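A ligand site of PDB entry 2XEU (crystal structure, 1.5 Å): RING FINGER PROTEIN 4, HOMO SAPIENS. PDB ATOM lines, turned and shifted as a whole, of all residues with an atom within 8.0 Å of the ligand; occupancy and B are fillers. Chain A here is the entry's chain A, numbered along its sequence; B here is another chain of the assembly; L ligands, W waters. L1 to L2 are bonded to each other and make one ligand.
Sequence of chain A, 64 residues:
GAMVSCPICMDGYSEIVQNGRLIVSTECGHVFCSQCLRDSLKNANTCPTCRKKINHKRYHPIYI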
ATOM      1  N   GLY A   1     -33.796  19.717  16.021  1.00  0.00           N
ATOM      2  CA  GLY A   1     -33.108  20.628  15.081  1.00  0.00           C
ATOM      3  C   GLY A   1     -33.942  21.845  14.750  1.00  0.00           C
ATOM      4  O   GLY A   1     -35.167  21.780  14.671  1.00  0.00           O
ATOM      5  N   ALA A   2     -33.259  22.960  14.566  1.00  0.00           N
ATOM      6  CA  ALA A   2     -33.897  24.208  14.258  1.00  0.00           C
ATOM      7  C   ALA A   2     -32.908  25.066  13.503  1.00  0.00           C
ATOM      8  O   ALA A   2     -31.716  24.754  13.435  1.00  0.00           O
ATOM      9  CB  ALA A   2     -34.317  24.921  15.549  1.00  0.00           C
ATOM     10  N   TYR A  13     -27.672  27.573  14.541  1.00  0.00           N
ATOM     11  CA  TYR A  13     -28.007  26.471  15.440  1.00  0.00           C
ATOM     12  C   TYR A  13     -27.023  25.316  15.331  1.00  0.00           C
ATOM     13  O   TYR A  13     -26.562  24.813  16.339  1.00  0.00           O
ATOM     14  CB  TYR A  13     -29.409  25.966  15.105  1.00  0.00           C
ATOM     15  CG  TYR A  13     -29.869  24.743  15.875  1.00  0.00           C
ATOM     16  CD1 TYR A  13     -30.570  24.869  17.060  1.00  0.00           C
ATOM     17  CD2 TYR A  13     -29.612  23.467  15.390  1.00  0.00           C
ATOM     18  CE1 TYR A  13     -31.013  23.753  17.752  1.00  0.00           C
ATOM     19  CE2 TYR A  13     -30.027  22.348  16.074  1.00  0.00           C
ATOM     20  CZ  TYR A  13     -30.728  22.491  17.255  1.00  0.00           C
ATOM     21  OH  TYR A  13     -31.169  21.360  17.906  1.00  0.00           O
ATOM     22  N   ILE A  16     -23.822  26.135  17.105  1.00  0.00           N
ATOM     23  CA  ILE A  16     -24.055  26.257  18.545  1.00  0.00           C
ATOM     24  C   ILE A  16     -24.129  24.874  19.202  1.00  0.00           C
ATOM     25  O   ILE A  16     -23.454  24.611  20.192  1.00  0.00           O
ATOM     26  CB  ILE A  16     -25.352  27.034  18.836  1.00  0.00           C
ATOM     27  CG1 ILE A  16     -25.201  28.507  18.429  1.00  0.00           C
ATOM     28  CG2 ILE A  16     -25.732  26.961  20.300  1.00  0.00           C
ATOM     29  CD1 ILE A  16     -26.520  29.236  18.340  1.00  0.00           C
ATOM     30  N   VAL A  17     -24.961  24.007  18.646  1.00  0.00           N
ATOM     31  CA  VAL A  17     -25.150  22.693  19.239  1.00  0.00           C
ATOM     32  C   VAL A  17     -23.943  21.760  18.976  1.00  0.00           C
ATOM     33  O   VAL A  17     -23.647  20.916  19.807  1.00  0.00           O
ATOM     34  CB  VAL A  17     -26.495  22.028  18.803  1.00  0.00           C
ATOM     35  CG1 VAL A  17     -27.664  22.947  19.151  1.00  0.00           C
ATOM     36  CG2 VAL A  17     -26.485  21.684  17.323  1.00  0.00           C
ATOM     37  N   GLN A  18     -23.245  21.950  17.863  1.00  0.00           N
ATOM     38  CA  GLN A  18     -22.004  21.183  17.579  1.00  0.00           C
ATOM     39  C   GLN A  18     -20.954  21.387  18.686  1.00  0.00           C
ATOM     40  O   GLN A  18     -20.160  20.482  18.969  1.00  0.00           O
ATOM     41  CB  GLN A  18     -21.402  21.575  16.222  1.00  0.00           C
ATOM     42  CG  GLN A  18     -20.107  20.831  15.834  1.00  0.00           C
ATOM     43  CD  GLN A  18     -19.336  21.501  14.692  1.00  0.00           C
ATOM     44  OE1 GLN A  18     -19.453  22.709  14.453  1.00  0.00           O
ATOM     45  NE2 GLN A  18     -18.529  20.707  13.982  1.00  0.00           N
ATOM     46  N   ASN A  19     -20.958  22.586  19.253  1.00  0.00           N
ATOM     47  CA  ASN A  19     -20.030  23.029  20.288  1.00  0.00           C
ATOM     48  C   ASN A  19     -20.523  22.753  21.719  1.00  0.00           C
ATOM     49  O   ASN A  19     -19.972  23.275  22.679  1.00  0.00           O
ATOM     50  CB  ASN A  19     -19.828  24.547  20.083  1.00  0.00           C
ATOM     51  CG  ASN A  19     -18.608  25.097  20.790  1.00  0.00           C
ATOM     52  OD1 ASN A  19     -18.713  26.068  21.547  1.00  0.00           O
ATOM     53  ND2 ASN A  19     -17.449  24.500  20.539  1.00  0.00           N
ATOM     54  N   GLY A  20     -21.598  21.982  21.880  1.00  0.00           N
ATOM     55  CA  GLY A  20     -22.104  21.646  23.217  1.00  0.00           C
ATOM     56  C   GLY A  20     -22.858  22.748  23.969  1.00  0.00           C
ATOM     57  O   GLY A  20     -23.120  22.621  25.175  1.00  0.00           O
ATOM     58  N   ARG A  21     -23.193  23.828  23.270  1.00  0.00           N
ATOM     59  CA  ARG A  21     -23.947  24.911  23.877  1.00  0.00           C
ATOM     60  C   ARG A  21     -25.435  24.611  23.796  1.00  0.00           C
ATOM     61  O   ARG A  21     -25.880  23.772  23.011  1.00  0.00           O
ATOM     62  CB  ARG A  21     -23.617  26.243  23.201  1.00  0.00           C
ATOM     63  CG  ARG A  21     -22.250  26.793  23.578  1.00  0.00           C
ATOM     64  CD  ARG A  21     -21.881  28.015  22.750  1.00  0.00           C
ATOM     65  NE  ARG A  21     -21.535  27.666  21.377  1.00  0.00           N
ATOM     66  CZ  ARG A  21     -21.467  28.532  20.365  1.00  0.00           C
ATOM     67  NH1 ARG A  21     -21.744  29.820  20.532  1.00  0.00           N
ATOM     68  NH2 ARG A  21     -21.136  28.098  19.149  1.00  0.00           N
ATOM     69  N   LEU A  22     -26.188  25.291  24.655  1.00  0.00           N
ATOM     70  CA  LEU A  22     -27.640  25.232  24.634  1.00  0.00           C
ATOM     71  C   LEU A  22     -28.192  26.451  23.930  1.00  0.00           C
ATOM     72  O   LEU A  22     -27.553  27.505  23.919  1.00  0.00           O
ATOM     73  CB  LEU A  22     -28.196  25.207  26.062  1.00  0.00           C
ATOM     74  CG  LEU A  22     -27.851  23.987  26.919  1.00  0.00           C
ATOM     75  CD1 LEU A  22     -28.100  24.271  28.395  1.00  0.00           C
ATOM     76  CD2 LEU A  22     -28.665  22.798  26.468  1.00  0.00           C
ATOM     77  N   ILE A  23     -29.366  26.316  23.351  1.00  0.00           N
ATOM     78  CA  ILE A  23     -30.149  27.482  22.962  1.00  0.00           C
ATOM     79  C   ILE A  23     -30.914  27.887  24.226  1.00  0.00           C
ATOM     80  O   ILE A  23     -31.505  27.044  24.891  1.00  0.00           O
ATOM     81  CB  ILE A  23     -31.131  27.184  21.817  1.00  0.00           C
ATOM     82  CG1 ILE A  23     -30.456  26.475  20.635  1.00  0.00           C
ATOM     83  CG2 ILE A  23     -31.790  28.481  21.345  1.00  0.00           C
ATOM     84  CD1 ILE A  23     -29.380  27.250  19.977  1.00  0.00           C
ATOM     85  N   VAL A  24     -30.882  29.166  24.562  1.00  0.00           N
ATOM     86  CA  VAL A  24     -31.571  29.664  25.749  1.00  0.00           C
ATOM     87  C   VAL A  24     -32.435  30.855  25.403  1.00  0.00           C
ATOM     88  O   VAL A  24     -32.188  31.562  24.430  1.00  0.00           O
ATOM     89  CB  VAL A  24     -30.587  30.051  26.868  1.00  0.00           C
ATOM     90  CG1 VAL A  24     -29.715  28.843  27.249  1.00  0.00           C
ATOM     91  CG2 VAL A  24     -29.714  31.232  26.474  1.00  0.00           C
ATOM     92  N   SER A  34     -26.102  29.666  25.104  1.00  0.00           N
ATOM     93  CA  SER A  34     -25.843  29.692  26.537  1.00  0.00           C
ATOM     94  C   SER A  34     -24.543  30.392  26.932  1.00  0.00           C
ATOM     95  O   SER A  34     -24.485  31.078  27.945  1.00  0.00           O
ATOM     96  CB  SER A  34     -25.874  28.276  27.099  1.00  0.00           C
ATOM     97  OG  SER A  34     -25.036  27.386  26.358  1.00  0.00           O
ATOM     98  N   PRO A  61     -33.088  27.023  29.170  1.00  0.00           N
ATOM     99  CA  PRO A  61     -32.932  26.433  27.844  1.00  0.00           C
ATOM    100  C   PRO A  61     -34.247  26.363  27.092  1.00  0.00           C
ATOM    101  O   PRO A  61     -35.338  26.306  27.709  1.00  0.00           O
ATOM    102  CB  PRO A  61     -32.424  25.021  28.150  1.00  0.00           C
ATOM    103  CG  PRO A  61     -31.945  25.053  29.520  1.00  0.00           C
ATOM    104  CD  PRO A  61     -32.745  26.084  30.239  1.00  0.00           C
ATOM    105  N   ILE A  62     -34.159  26.367  25.769  1.00  0.00           N
ATOM    106  CA  ILE A  62     -35.266  25.987  24.911  1.00  0.00           C
ATOM    107  C   ILE A  62     -34.808  24.799  24.044  1.00  0.00           C
ATOM    108  O   ILE A  62     -33.775  24.838  23.388  1.00  0.00           O
ATOM    109  CB  ILE A  62     -35.830  27.153  24.060  1.00  0.00           C
ATOM    110  CG1 ILE A  62     -34.766  27.779  23.142  1.00  0.00           C
ATOM    111  CG2 ILE A  62     -36.462  28.219  24.958  1.00  0.00           C
ATOM    112  CD1 ILE A  62     -35.354  28.796  22.192  1.00  0.00           C
ATOM    113  N   TYR A  63     -35.593  23.741  24.089  1.00  0.00           N
ATOM    114  CA  TYR A  63     -35.224  22.491  23.497  1.00  0.00           C
ATOM    115  C   TYR A  63     -35.798  22.405  22.102  1.00  0.00           C
ATOM    116  O   TYR A  63     -36.914  21.930  21.893  1.00  0.00           O
ATOM    117  CB  TYR A  63     -35.701  21.351  24.380  1.00  0.00           C
ATOM    118  CG  TYR A  63     -35.042  21.388  25.730  1.00  0.00           C
ATOM    119  CD1 TYR A  63     -33.692  21.125  25.851  1.00  0.00           C
ATOM    120  CD2 TYR A  63     -35.755  21.713  26.876  1.00  0.00           C
ATOM    121  CE1 TYR A  63     -33.070  21.178  27.071  1.00  0.00           C
ATOM    122  CE2 TYR A  63     -35.137  21.753  28.113  1.00  0.00           C
ATOM    123  CZ  TYR A  63     -33.791  21.482  28.197  1.00  0.00           C
ATOM    124  OH  TYR A  63     -33.140  21.528  29.419  1.00  0.00           O
ATOM    125  N   ILE A  64     -34.999  22.872  21.152  1.00  0.00           N
ATOM    126  CA  ILE A  64     -35.407  22.900  19.747  1.00  0.00           C
ATOM    127  C   ILE A  64     -34.359  22.250  18.875  1.00  0.00           C
ATOM    128  O   ILE A  64     -34.589  22.048  17.681  1.00  0.00           O
ATOM    129  CB  ILE A  64     -35.685  24.352  19.255  1.00  0.00           C
ATOM    130  CG1 ILE A  64     -34.433  25.244  19.345  1.00  0.00           C
ATOM    131  CG2 ILE A  64     -36.847  24.948  20.039  1.00  0.00           C
ATOM    132  CD1 ILE A  64     -34.630  26.654  18.814  1.00  0.00           C
ATOM    133  OXT ILE A  64     -33.269  21.886  19.329  1.00  0.00           O
ATOM    134  N   GLY B  29     -38.778  24.799  28.819  1.00  0.00           N
ATOM    135  CA  GLY B  29     -38.049  24.835  27.569  1.00  0.00           C
ATOM    136  C   GLY B  29     -38.727  24.205  26.373  1.00  0.00           C
ATOM    137  O   GLY B  29     -38.088  23.939  25.353  1.00  0.00           O
ATOM    138  N   HIS B  30     -40.030  23.968  26.469  1.00  0.00           N
ATOM    139  CA  HIS B  30     -40.767  23.321  25.404  1.00  0.00           C
ATOM    140  C   HIS B  30     -41.522  24.339  24.564  1.00  0.00           C
ATOM    141  O   HIS B  30     -42.247  25.194  25.102  1.00  0.00           O
ATOM    142  CB  HIS B  30     -41.596  22.196  25.995  1.00  0.00           C
ATOM    143  CG  HIS B  30     -40.732  21.151  26.614  1.00  0.00           C
ATOM    144  ND1 HIS B  30     -40.825  20.763  27.938  1.00  0.00           N
ATOM    145  CD2 HIS B  30     -39.655  20.505  26.111  1.00  0.00           C
ATOM    146  CE1 HIS B  30     -39.865  19.886  28.193  1.00  0.00           C
ATOM    147  NE2 HIS B  30     -39.142  19.718  27.097  1.00  0.00           N
HETATM  148  C1  LIG L   1     -30.073  17.494  23.718  1.00  0.00           C
HETATM  149  C2  LIG L   1     -30.699  16.653  24.812  1.00  0.00           C
HETATM  150  C3  LIG L   1     -30.939  17.497  26.064  1.00  0.00           C
HETATM  151  C4  LIG L   1     -29.643  18.181  26.498  1.00  0.00           C
HETATM  152  C5  LIG L   1     -29.049  18.969  25.342  1.00  0.00           C
HETATM  153  C6  LIG L   1     -27.676  19.552  25.675  1.00  0.00           C
HETATM  154  O1  LIG L   1     -31.906  16.074  24.338  1.00  0.00           O
HETATM  155  O2  LIG L   1     -31.436  16.687  27.106  1.00  0.00           O
HETATM  156  O3  LIG L   1     -29.864  19.054  27.577  1.00  0.00           O
HETATM  157  O4  LIG L   1     -28.912  18.155  24.209  1.00  0.00           O
HETATM  158  O5  LIG L   1     -26.722  18.540  25.936  1.00  0.00           O
HETATM  159  C1  LG2 L   2     -31.038  17.801  20.917  1.00  0.00           C
HETATM  160  C2  LG2 L   2     -30.926  18.921  21.929  1.00  0.00           C
HETATM  161  C3  LG2 L   2     -32.002  19.983  21.710  1.00  0.00           C
HETATM  162  C4  LG2 L   2     -31.285  21.218  22.219  1.00  0.00           C
HETATM  163  C5  LG2 L   2     -29.848  20.965  21.757  1.00  0.00           C
HETATM  164  C6  LG2 L   2     -28.843  21.627  22.671  1.00  0.00           C
HETATM  165  O1  LG2 L   2     -30.971  18.296  19.593  1.00  0.00           O
HETATM  166  O2  LG2 L   2     -31.033  18.431  23.265  1.00  0.00           O
HETATM  167  O3  LG2 L   2     -33.196  19.697  22.391  1.00  0.00           O
HETATM  168  O4  LG2 L   2     -31.846  22.410  21.719  1.00  0.00           O
HETATM  169  O5  LG2 L   2     -29.676  19.563  21.754  1.00  0.00           O
HETATM  170  O6  LG2 L   2     -27.515  21.392  22.210  1.00  0.00           O
HETATM  171  O   HOH W   1     -29.635  19.131  17.698  1.00  0.00           O
HETATM  172  O   HOH W   2     -26.002  18.325  28.728  1.00  0.00           O
HETATM  173  O   HOH W   3     -31.110  24.138  23.726  1.00  0.00           O
HETATM  174  O   HOH W   4     -34.504  17.886  27.376  1.00  0.00           O
HETATM  175  O   HOH W   5     -34.147  14.705  26.952  1.00  0.00           O
HETATM  176  O   HOH W   6     -24.683  20.403  26.246  1.00  0.00           O
HETATM  177  O   HOH W   7     -34.191  17.825  24.516  1.00  0.00           O
HETATM  178  O   HOH W   8     -32.286  18.923  29.404  1.00  0.00           O
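Water W1 bridges O1 of LG2 L2 (2.5 Å) and OH of Tyr 13 (2.7 Å).
Water W3 lies within hydrogen-bond range of O4 of LG2 L2, O of Ile 62 and N of Ile 23.
Water W6 bridges O5 of LIG L1 (2.8 Å) and O of Gly 20 (2.9 Å).
Water W8 lies within hydrogen-bond range of OH of Tyr 63 (2.7 Å) and O3 of LIG L1 (3.0 Å).
N of Tyr 63 is in hydrogen-bond range of O of Gly 29 of chain B (2.8 Å).
O of Leu 22 is in hydrogen-bond range of N of Ser 34, 2.9 Å away.
The chain-end carboxylate of Ile 64 sits at hydrogen-bond distance from the side-chain hydroxyl of Tyr 13 (2.6 Å).
The backbone carbonyl oxygen of Ile 16 sits at hydrogen-bond distance from the backbone NH of Arg 21 (3.2 Å).
The backbone NH (N) of Gly 1 is in hydrogen-bond range of the chain-end carboxylate (O) of Ile 64 (3.0 Å).
The backbone carbonyl oxygen of Ile 23 lies within hydrogen-bond range of the backbone NH of Ile 62 (2.9 Å).
NE of Arg 21 is in hydrogen-bond range of OD1 of Asn 19, at 3.2 Å.
An oxygen (O4) of LG2 L2 sits at hydrogen-bond distance from the chain-end carboxylate (OXT) of Ile 64 (2.8 Å).
An oxygen (O6) of LG2 L2 lies within hydrogen-bond range of the backbone carbonyl oxygen (O) of Arg 21 (3.0 Å).
N of Ile 64 lies within hydrogen-bond range of O4 of LG2 L2 (3.2 Å).
Residues that only touch the ligand: Val 17, Leu 22, Tyr 13, Ile 62 and Tyr 63.
Hydrophobic or aromatic side chains within 4 Å of the ligand: Val 17, Leu 22 and Tyr 63.
Within 4 Å of the ligand: Tyr 13, Val 17, Arg 21, Leu 22, Ile 62, Tyr 63 and Ile 64.
Along chain A the residues within 4 Å of the ligand span positions 13 to 64.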
